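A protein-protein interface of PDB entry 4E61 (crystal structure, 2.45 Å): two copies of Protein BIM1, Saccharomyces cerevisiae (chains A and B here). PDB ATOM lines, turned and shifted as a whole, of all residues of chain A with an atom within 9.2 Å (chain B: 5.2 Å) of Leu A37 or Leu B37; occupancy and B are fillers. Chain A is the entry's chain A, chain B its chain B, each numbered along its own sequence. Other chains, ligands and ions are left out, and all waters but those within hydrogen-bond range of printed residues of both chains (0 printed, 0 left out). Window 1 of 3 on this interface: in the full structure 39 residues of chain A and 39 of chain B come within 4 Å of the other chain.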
ATOM      1  N   GLN A  29      33.543  16.725  -2.393  1.00  0.00           N
ATOM      2  CA  GLN A  29      32.386  15.868  -2.637  1.00  0.00           C
ATOM      3  C   GLN A  29      31.599  16.395  -3.856  1.00  0.00           C
ATOM      4  O   GLN A  29      31.329  15.618  -4.778  1.00  0.00           O
ATOM      5  CB  GLN A  29      31.476  15.804  -1.397  1.00  0.00           C
ATOM      6  CG  GLN A  29      31.336  14.412  -0.805  1.00  0.00           C
ATOM      7  CD  GLN A  29      32.354  14.144   0.271  1.00  0.00           C
ATOM      8  OE1 GLN A  29      32.062  14.257   1.470  1.00  0.00           O
ATOM      9  NE2 GLN A  29      33.569  13.772  -0.131  1.00  0.00           N
ATOM     10  N   TYR A  30      31.293  17.726  -3.872  1.00  0.00           N
ATOM     11  CA  TYR A  30      30.567  18.433  -4.941  1.00  0.00           C
ATOM     12  C   TYR A  30      31.296  18.391  -6.269  1.00  0.00           C
ATOM     13  O   TYR A  30      30.652  18.234  -7.303  1.00  0.00           O
ATOM     14  CB  TYR A  30      30.217  19.872  -4.560  1.00  0.00           C
ATOM     15  CG  TYR A  30      28.974  19.998  -3.700  1.00  0.00           C
ATOM     16  CD1 TYR A  30      27.711  19.721  -4.218  1.00  0.00           C
ATOM     17  CD2 TYR A  30      29.055  20.444  -2.380  1.00  0.00           C
ATOM     18  CE1 TYR A  30      26.565  19.840  -3.430  1.00  0.00           C
ATOM     19  CE2 TYR A  30      27.917  20.577  -1.587  1.00  0.00           C
ATOM     20  CZ  TYR A  30      26.673  20.272  -2.113  1.00  0.00           C
ATOM     21  OH  TYR A  30      25.560  20.403  -1.311  1.00  0.00           O
ATOM     22  N   LYS A  31      32.639  18.505  -6.244  1.00  0.00           N
ATOM     23  CA  LYS A  31      33.496  18.420  -7.435  1.00  0.00           C
ATOM     24  C   LYS A  31      33.386  17.009  -8.053  1.00  0.00           C
ATOM     25  O   LYS A  31      33.390  16.874  -9.273  1.00  0.00           O
ATOM     26  CB  LYS A  31      34.961  18.716  -7.076  1.00  0.00           C
ATOM     27  CG  LYS A  31      35.316  20.195  -6.947  1.00  0.00           C
ATOM     28  CD  LYS A  31      36.769  20.339  -6.489  1.00  0.00           C
ATOM     29  CE  LYS A  31      37.255  21.763  -6.430  1.00  0.00           C
ATOM     30  NZ  LYS A  31      38.651  21.833  -5.928  1.00  0.00           N
ATOM     31  N   GLY A  32      33.287  15.999  -7.187  1.00  0.00           N
ATOM     32  CA  GLY A  32      33.118  14.595  -7.520  1.00  0.00           C
ATOM     33  C   GLY A  32      31.741  14.329  -8.100  1.00  0.00           C
ATOM     34  O   GLY A  32      31.624  13.541  -9.037  1.00  0.00           O
ATOM     35  N   THR A  33      30.686  14.983  -7.563  1.00  0.00           N
ATOM     36  CA  THR A  33      29.337  14.825  -8.105  1.00  0.00           C
ATOM     37  C   THR A  33      29.142  15.528  -9.457  1.00  0.00           C
ATOM     38  O   THR A  33      28.423  14.993 -10.296  1.00  0.00           O
ATOM     39  CB  THR A  33      28.172  14.916  -7.079  1.00  0.00           C
ATOM     40  OG1 THR A  33      26.958  15.279  -7.754  1.00  0.00           O
ATOM     41  CG2 THR A  33      28.408  15.900  -5.986  1.00  0.00           C
ATOM     42  N   VAL A  34      29.810  16.680  -9.687  1.00  0.00           N
ATOM     43  CA  VAL A  34      29.732  17.406 -10.965  1.00  0.00           C
ATOM     44  C   VAL A  34      30.461  16.571 -12.044  1.00  0.00           C
ATOM     45  O   VAL A  34      29.927  16.384 -13.143  1.00  0.00           O
ATOM     46  CB  VAL A  34      30.259  18.875 -10.864  1.00  0.00           C
ATOM     47  CG1 VAL A  34      30.513  19.479 -12.247  1.00  0.00           C
ATOM     48  CG2 VAL A  34      29.298  19.751 -10.068  1.00  0.00           C
ATOM     49  N   SER A  35      31.652  16.042 -11.695  1.00  0.00           N
ATOM     50  CA  SER A  35      32.488  15.195 -12.553  1.00  0.00           C
ATOM     51  C   SER A  35      31.746  13.922 -13.025  1.00  0.00           C
ATOM     52  O   SER A  35      31.816  13.619 -14.212  1.00  0.00           O
ATOM     53  CB  SER A  35      33.782  14.818 -11.841  1.00  0.00           C
ATOM     54  OG  SER A  35      34.655  14.145 -12.728  1.00  0.00           O
ATOM     55  N   THR A  36      31.022  13.210 -12.118  1.00  0.00           N
ATOM     56  CA  THR A  36      30.245  12.014 -12.456  1.00  0.00           C
ATOM     57  C   THR A  36      29.115  12.381 -13.453  1.00  0.00           C
ATOM     58  O   THR A  36      28.957  11.692 -14.466  1.00  0.00           O
ATOM     59  CB  THR A  36      29.736  11.265 -11.196  1.00  0.00           C
ATOM     60  OG1 THR A  36      30.817  10.645 -10.514  1.00  0.00           O
ATOM     61  CG2 THR A  36      28.693  10.227 -11.509  1.00  0.00           C
ATOM     62  N   LEU A  37      28.371  13.467 -13.169  1.00  0.00           N
ATOM     63  CA  LEU A  37      27.287  13.957 -14.002  1.00  0.00           C
ATOM     64  C   LEU A  37      27.778  14.373 -15.395  1.00  0.00           C
ATOM     65  O   LEU A  37      27.080  14.134 -16.389  1.00  0.00           O
ATOM     66  CB  LEU A  37      26.531  15.101 -13.311  1.00  0.00           C
ATOM     67  CG  LEU A  37      25.639  14.727 -12.116  1.00  0.00           C
ATOM     68  CD1 LEU A  37      25.329  15.958 -11.262  1.00  0.00           C
ATOM     69  CD2 LEU A  37      24.336  14.069 -12.570  1.00  0.00           C
ATOM     70  N   GLU A  38      28.994  14.932 -15.476  1.00  0.00           N
ATOM     71  CA  GLU A  38      29.597  15.334 -16.754  1.00  0.00           C
ATOM     72  C   GLU A  38      30.119  14.141 -17.562  1.00  0.00           C
ATOM     73  O   GLU A  38      30.111  14.188 -18.794  1.00  0.00           O
ATOM     74  CB  GLU A  38      30.692  16.391 -16.549  1.00  0.00           C
ATOM     75  CG  GLU A  38      30.117  17.763 -16.232  1.00  0.00           C
ATOM     76  CD  GLU A  38      31.103  18.846 -15.835  1.00  0.00           C
ATOM     77  OE1 GLU A  38      32.276  18.520 -15.537  1.00  0.00           O
ATOM     78  OE2 GLU A  38      30.689  20.027 -15.803  1.00  0.00           O
ATOM     79  N   ILE A  39      30.562  13.071 -16.866  1.00  0.00           N
ATOM     80  CA  ILE A  39      31.035  11.828 -17.489  1.00  0.00           C
ATOM     81  C   ILE A  39      29.839  11.093 -18.081  1.00  0.00           C
ATOM     82  O   ILE A  39      29.957  10.640 -19.209  1.00  0.00           O
ATOM     83  CB  ILE A  39      31.898  10.945 -16.545  1.00  0.00           C
ATOM     84  CG1 ILE A  39      33.273  11.604 -16.268  1.00  0.00           C
ATOM     85  CG2 ILE A  39      32.087   9.538 -17.117  1.00  0.00           C
ATOM     86  CD1 ILE A  39      33.970  11.072 -14.970  1.00  0.00           C
ATOM     87  N   GLU A  40      28.682  11.035 -17.349  1.00  0.00           N
ATOM     88  CA  GLU A  40      27.426  10.415 -17.782  1.00  0.00           C
ATOM     89  C   GLU A  40      26.956  11.065 -19.061  1.00  0.00           C
ATOM     90  O   GLU A  40      26.643  10.377 -20.040  1.00  0.00           O
ATOM     91  CB  GLU A  40      26.329  10.605 -16.741  1.00  0.00           C
ATOM     92  CG  GLU A  40      26.403   9.690 -15.538  1.00  0.00           C
ATOM     93  CD  GLU A  40      25.293   9.845 -14.517  1.00  0.00           C
ATOM     94  OE1 GLU A  40      25.088   8.898 -13.724  1.00  0.00           O
ATOM     95  OE2 GLU A  40      24.612  10.898 -14.518  1.00  0.00           O
ATOM     96  N   ARG A  41      26.935  12.387 -19.037  1.00  0.00           N
ATOM     97  CA  ARG A  41      26.540  13.287 -20.091  1.00  0.00           C
ATOM     98  C   ARG A  41      27.284  13.033 -21.395  1.00  0.00           C
ATOM     99  O   ARG A  41      26.639  12.867 -22.434  1.00  0.00           O
ATOM    100  CB  ARG A  41      26.771  14.703 -19.603  1.00  0.00           C
ATOM    101  CG  ARG A  41      25.683  15.666 -20.015  1.00  0.00           C
ATOM    102  CD  ARG A  41      26.188  16.630 -21.056  1.00  0.00           C
ATOM    103  NE  ARG A  41      27.344  17.414 -20.612  1.00  0.00           N
ATOM    104  CZ  ARG A  41      27.267  18.517 -19.876  1.00  0.00           C
ATOM    105  NH1 ARG A  41      26.089  18.964 -19.457  1.00  0.00           N
ATOM    106  NH2 ARG A  41      28.369  19.176 -19.545  1.00  0.00           N
ATOM    107  N   GLU A  42      28.625  12.953 -21.338  1.00  0.00           N
ATOM    108  CA  GLU A  42      29.438  12.679 -22.521  1.00  0.00           C
ATOM    109  C   GLU A  42      29.078  11.310 -23.123  1.00  0.00           C
ATOM    110  O   GLU A  42      28.985  11.186 -24.338  1.00  0.00           O
ATOM    111  CB  GLU A  42      30.945  12.757 -22.190  1.00  0.00           C
ATOM    112  N   PHE A  43      28.824  10.311 -22.272  1.00  0.00           N
ATOM    113  CA  PHE A  43      28.473   8.958 -22.682  1.00  0.00           C
ATOM    114  C   PHE A  43      27.080   8.897 -23.327  1.00  0.00           C
ATOM    115  O   PHE A  43      26.934   8.350 -24.416  1.00  0.00           O
ATOM    116  CB  PHE A  43      28.659   7.993 -21.506  1.00  0.00           C
ATOM    117  CG  PHE A  43      28.321   6.547 -21.766  1.00  0.00           C
ATOM    118  CD1 PHE A  43      29.093   5.768 -22.634  1.00  0.00           C
ATOM    119  CD2 PHE A  43      27.252   5.950 -21.123  1.00  0.00           C
ATOM    120  CE1 PHE A  43      28.782   4.425 -22.864  1.00  0.00           C
ATOM    121  CE2 PHE A  43      26.968   4.596 -21.323  1.00  0.00           C
ATOM    122  CZ  PHE A  43      27.757   3.837 -22.167  1.00  0.00           C
ATOM    123  N   TYR A  44      26.075   9.511 -22.688  1.00  0.00           N
ATOM    124  CA  TYR A  44      24.733   9.532 -23.261  1.00  0.00           C
ATOM    125  C   TYR A  44      24.585  10.459 -24.484  1.00  0.00           C
ATOM    126  O   TYR A  44      23.824  10.122 -25.397  1.00  0.00           O
ATOM    127  CB  TYR A  44      23.582   9.570 -22.215  1.00  0.00           C
ATOM    128  CG  TYR A  44      23.415  10.837 -21.405  1.00  0.00           C
ATOM    129  CD1 TYR A  44      22.985  12.021 -22.003  1.00  0.00           C
ATOM    130  CD2 TYR A  44      23.533  10.821 -20.018  1.00  0.00           C
ATOM    131  CE1 TYR A  44      22.807  13.186 -21.260  1.00  0.00           C
ATOM    132  CE2 TYR A  44      23.340  11.979 -19.258  1.00  0.00           C
ATOM    133  CZ  TYR A  44      22.963  13.159 -19.882  1.00  0.00           C
ATOM    134  OH  TYR A  44      22.776  14.317 -19.150  1.00  0.00           O
ATOM    135  N   PHE A  45      25.409  11.535 -24.569  1.00  0.00           N
ATOM    136  CA  PHE A  45      25.454  12.406 -25.754  1.00  0.00           C
ATOM    137  C   PHE A  45      26.033  11.670 -26.947  1.00  0.00           C
ATOM    138  O   PHE A  45      25.479  11.787 -28.051  1.00  0.00           O
ATOM    139  CB  PHE A  45      26.200  13.731 -25.506  1.00  0.00           C
ATOM    140  CG  PHE A  45      25.344  14.836 -24.922  1.00  0.00           C
ATOM    141  CD1 PHE A  45      23.990  14.641 -24.686  1.00  0.00           C
ATOM    142  CD2 PHE A  45      25.887  16.077 -24.634  1.00  0.00           C
ATOM    143  CE1 PHE A  45      23.203  15.661 -24.143  1.00  0.00           C
ATOM    144  CE2 PHE A  45      25.087  17.110 -24.124  1.00  0.00           C
ATOM    145  CZ  PHE A  45      23.757  16.883 -23.848  1.00  0.00           C
ATOM    146  N   THR B  33      25.055  24.209  -9.654  1.00  0.00           N
ATOM    147  CA  THR B  33      25.571  23.459 -10.798  1.00  0.00           C
ATOM    148  C   THR B  33      25.146  21.983 -10.789  1.00  0.00           C
ATOM    149  O   THR B  33      24.909  21.438 -11.864  1.00  0.00           O
ATOM    150  CB  THR B  33      27.016  23.786 -11.226  1.00  0.00           C
ATOM    151  OG1 THR B  33      27.528  22.706 -12.006  1.00  0.00           O
ATOM    152  CG2 THR B  33      27.952  24.006 -10.080  1.00  0.00           C
ATOM    153  N   VAL B  34      25.005  21.350  -9.599  1.00  0.00           N
ATOM    154  CA  VAL B  34      24.560  19.955  -9.475  1.00  0.00           C
ATOM    155  C   VAL B  34      23.073  19.891  -9.867  1.00  0.00           C
ATOM    156  O   VAL B  34      22.686  19.006 -10.634  1.00  0.00           O
ATOM    157  CB  VAL B  34      24.863  19.341  -8.081  1.00  0.00           C
ATOM    158  CG1 VAL B  34      24.066  18.064  -7.822  1.00  0.00           C
ATOM    159  CG2 VAL B  34      26.353  19.074  -7.910  1.00  0.00           C
ATOM    160  N   SER B  35      22.267  20.859  -9.386  1.00  0.00           N
ATOM    161  CA  SER B  35      20.831  20.982  -9.671  1.00  0.00           C
ATOM    162  C   SER B  35      20.541  21.105 -11.180  1.00  0.00           C
ATOM    163  O   SER B  35      19.649  20.411 -11.674  1.00  0.00           O
ATOM    164  CB  SER B  35      20.233  22.160  -8.911  1.00  0.00           C
ATOM    165  OG  SER B  35      18.824  22.179  -9.071  1.00  0.00           O
ATOM    166  N   THR B  36      21.309  21.959 -11.905  1.00  0.00           N
ATOM    167  CA  THR B  36      21.180  22.125 -13.359  1.00  0.00           C
ATOM    168  C   THR B  36      21.482  20.807 -14.107  1.00  0.00           C
ATOM    169  O   THR B  36      20.691  20.379 -14.955  1.00  0.00           O
ATOM    170  CB  THR B  36      21.917  23.381 -13.905  1.00  0.00           C
ATOM    171  OG1 THR B  36      21.772  23.372 -15.312  1.00  0.00           O
ATOM    172  CG2 THR B  36      23.407  23.436 -13.640  1.00  0.00           C
ATOM    173  N   LEU B  37      22.596  20.145 -13.731  1.00  0.00           N
ATOM    174  CA  LEU B  37      23.039  18.884 -14.304  1.00  0.00           C
ATOM    175  C   LEU B  37      22.047  17.773 -14.046  1.00  0.00           C
ATOM    176  O   LEU B  37      21.859  16.947 -14.923  1.00  0.00           O
ATOM    177  CB  LEU B  37      24.434  18.503 -13.807  1.00  0.00           C
ATOM    178  CG  LEU B  37      25.626  19.324 -14.339  1.00  0.00           C
ATOM    179  CD1 LEU B  37      26.845  19.143 -13.447  1.00  0.00           C
ATOM    180  CD2 LEU B  37      25.984  18.953 -15.787  1.00  0.00           C
ATOM    181  N   GLU B  38      21.380  17.775 -12.889  1.00  0.00           N
ATOM    182  CA  GLU B  38      20.356  16.785 -12.547  1.00  0.00           C
ATOM    183  C   GLU B  38      19.037  17.027 -13.287  1.00  0.00           C
ATOM    184  O   GLU B  38      18.320  16.068 -13.553  1.00  0.00           O
ATOM    185  CB  GLU B  38      20.131  16.700 -11.033  1.00  0.00           C
ATOM    186  CG  GLU B  38      21.250  15.961 -10.321  1.00  0.00           C
ATOM    187  CD  GLU B  38      21.222  15.961  -8.804  1.00  0.00           C
ATOM    188  OE1 GLU B  38      20.466  16.762  -8.206  1.00  0.00           O
ATOM    189  OE2 GLU B  38      21.988  15.168  -8.209  1.00  0.00           O
ATOM    190  N   ILE B  39      18.716  18.296 -13.610  1.00  0.00           N
ATOM    191  CA  ILE B  39      17.511  18.648 -14.363  1.00  0.00           C
ATOM    192  C   ILE B  39      17.690  18.204 -15.838  1.00  0.00           C
ATOM    193  O   ILE B  39      16.767  17.614 -16.413  1.00  0.00           O
ATOM    194  CB  ILE B  39      17.129  20.155 -14.205  1.00  0.00           C
ATOM    195  CG1 ILE B  39      16.606  20.448 -12.771  1.00  0.00           C
ATOM    196  CG2 ILE B  39      16.073  20.576 -15.253  1.00  0.00           C
ATOM    197  CD1 ILE B  39      16.710  21.931 -12.330  1.00  0.00           C
ATOM    198  N   GLU B  40      18.895  18.457 -16.410  1.00  0.00           N
ATOM    199  CA  GLU B  40      19.293  18.052 -17.762  1.00  0.00           C
ATOM    200  C   GLU B  40      19.231  16.522 -17.874  1.00  0.00           C
ATOM    201  O   GLU B  40      18.653  15.994 -18.819  1.00  0.00           O
ATOM    202  CB  GLU B  40      20.743  18.462 -18.053  1.00  0.00           C
ATOM    203  CG  GLU B  40      20.983  19.927 -18.356  1.00  0.00           C
ATOM    204  CD  GLU B  40      22.437  20.268 -18.659  1.00  0.00           C
ATOM    205  OE1 GLU B  40      23.189  19.379 -19.128  1.00  0.00           O
ATOM    206  OE2 GLU B  40      22.820  21.438 -18.433  1.00  0.00           O
ATOM    207  N   ARG B  41      19.811  15.823 -16.870  1.00  0.00           N
ATOM    208  CA  ARG B  41      19.897  14.364 -16.759  1.00  0.00           C
ATOM    209  C   ARG B  41      18.526  13.693 -16.777  1.00  0.00           C
ATOM    210  O   ARG B  41      18.380  12.675 -17.448  1.00  0.00           O
ATOM    211  CB  ARG B  41      20.702  13.976 -15.515  1.00  0.00           C
ATOM    212  CG  ARG B  41      21.042  12.507 -15.347  1.00  0.00           C
ATOM    213  CD  ARG B  41      21.134  12.239 -13.866  1.00  0.00           C
ATOM    214  NE  ARG B  41      21.694  10.932 -13.584  1.00  0.00           N
ATOM    215  CZ  ARG B  41      20.974   9.861 -13.289  1.00  0.00           C
ATOM    216  NH1 ARG B  41      19.648   9.931 -13.260  1.00  0.00           N
ATOM    217  NH2 ARG B  41      21.570   8.700 -13.048  1.00  0.00           N
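Of the printed residues of chain B, Tyr A30 touches Val B34.
Thr A36 touches none of the printed residues of chain B.
Of chain B, only Leu B37 and Arg B41 come within 4 Å of Leu A37.
Phe A43 touches none of the printed residues of chain B.
Of the printed residues of chain B, Tyr A44 touches Arg B41 (3.7 Å).
Printed residues of chain A within 4 Å of Thr B33: Val A34.
Printed residues of chain A within 4 Å of Val B34: Tyr A30 (3.99 Å), Thr A33 (3.8 Å) and Val A34 (3.7 Å).
No residue of chain A comes within 4 Å of Thr B36.
Glu B40 touches one residue of chain A.
The nearest residue of chain B that does not touch Leu A37 is Val B34 (4.1 Å).
The guanidinium group of Arg B41 is in salt-bridge range of the side-chain carboxylate of Glu A40.
The guanidinium group of Arg A41 lies within salt-bridge range of the side-chain carboxylate of Glu B40 (2.9 Å).
Among the printed residues, pairs that only touch across the chains: Arg A41 with Leu B37, Leu A37 with Leu B37, Val A34 with Val B34, Tyr A44 with Arg B41, Thr A33 with Val B34, Val A34 with Leu B37, Leu A37 with Arg B41, Val A34 with Thr B33 and Tyr A30 with Val B34.
Val A34 touches its own counterpart, Val B34.
Leu B37 touches its own counterpart, Leu A37.
Leu A37 touches Arg B41, and with the chains exchanged Arg A41 touches Leu B37.
Glu A40 touches Arg B41, and with the chains exchanged Arg A41 touches Glu B40.
Positions printed for both chains: 33, 34, 35, 36, 37, 38, 39, 40 and 41.
Of the 11 pairs that touch across the chains among the printed residues, 8 have their exchanged pair printed and touching as well.
Printed residues of chain B that touch a printed residue of chain A: Thr B33, Val B34, Leu B37, Glu B40 and Arg B41.
Hydrophobic or aromatic side chains of chain B that line the printed part of chain A: Val B34 and Leu B37.
Of the 17 printed residues of chain A, 7 touch a printed residue of chain B.
Printed residues of chain A that touch a printed residue of chain B: Tyr A30, Thr A33, Val A34, Leu A37, Glu A40, Arg A41 and Tyr A44.
Hydrophobic or aromatic side chains of chain A that line the printed part of chain B: Tyr A30, Val A34, Leu A37 and Tyr A44.
Along chain A the printed residues that touch a printed residue of chain B span positions 30 to 44.
Among the printed residues, 11 pairs touch across the chains.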
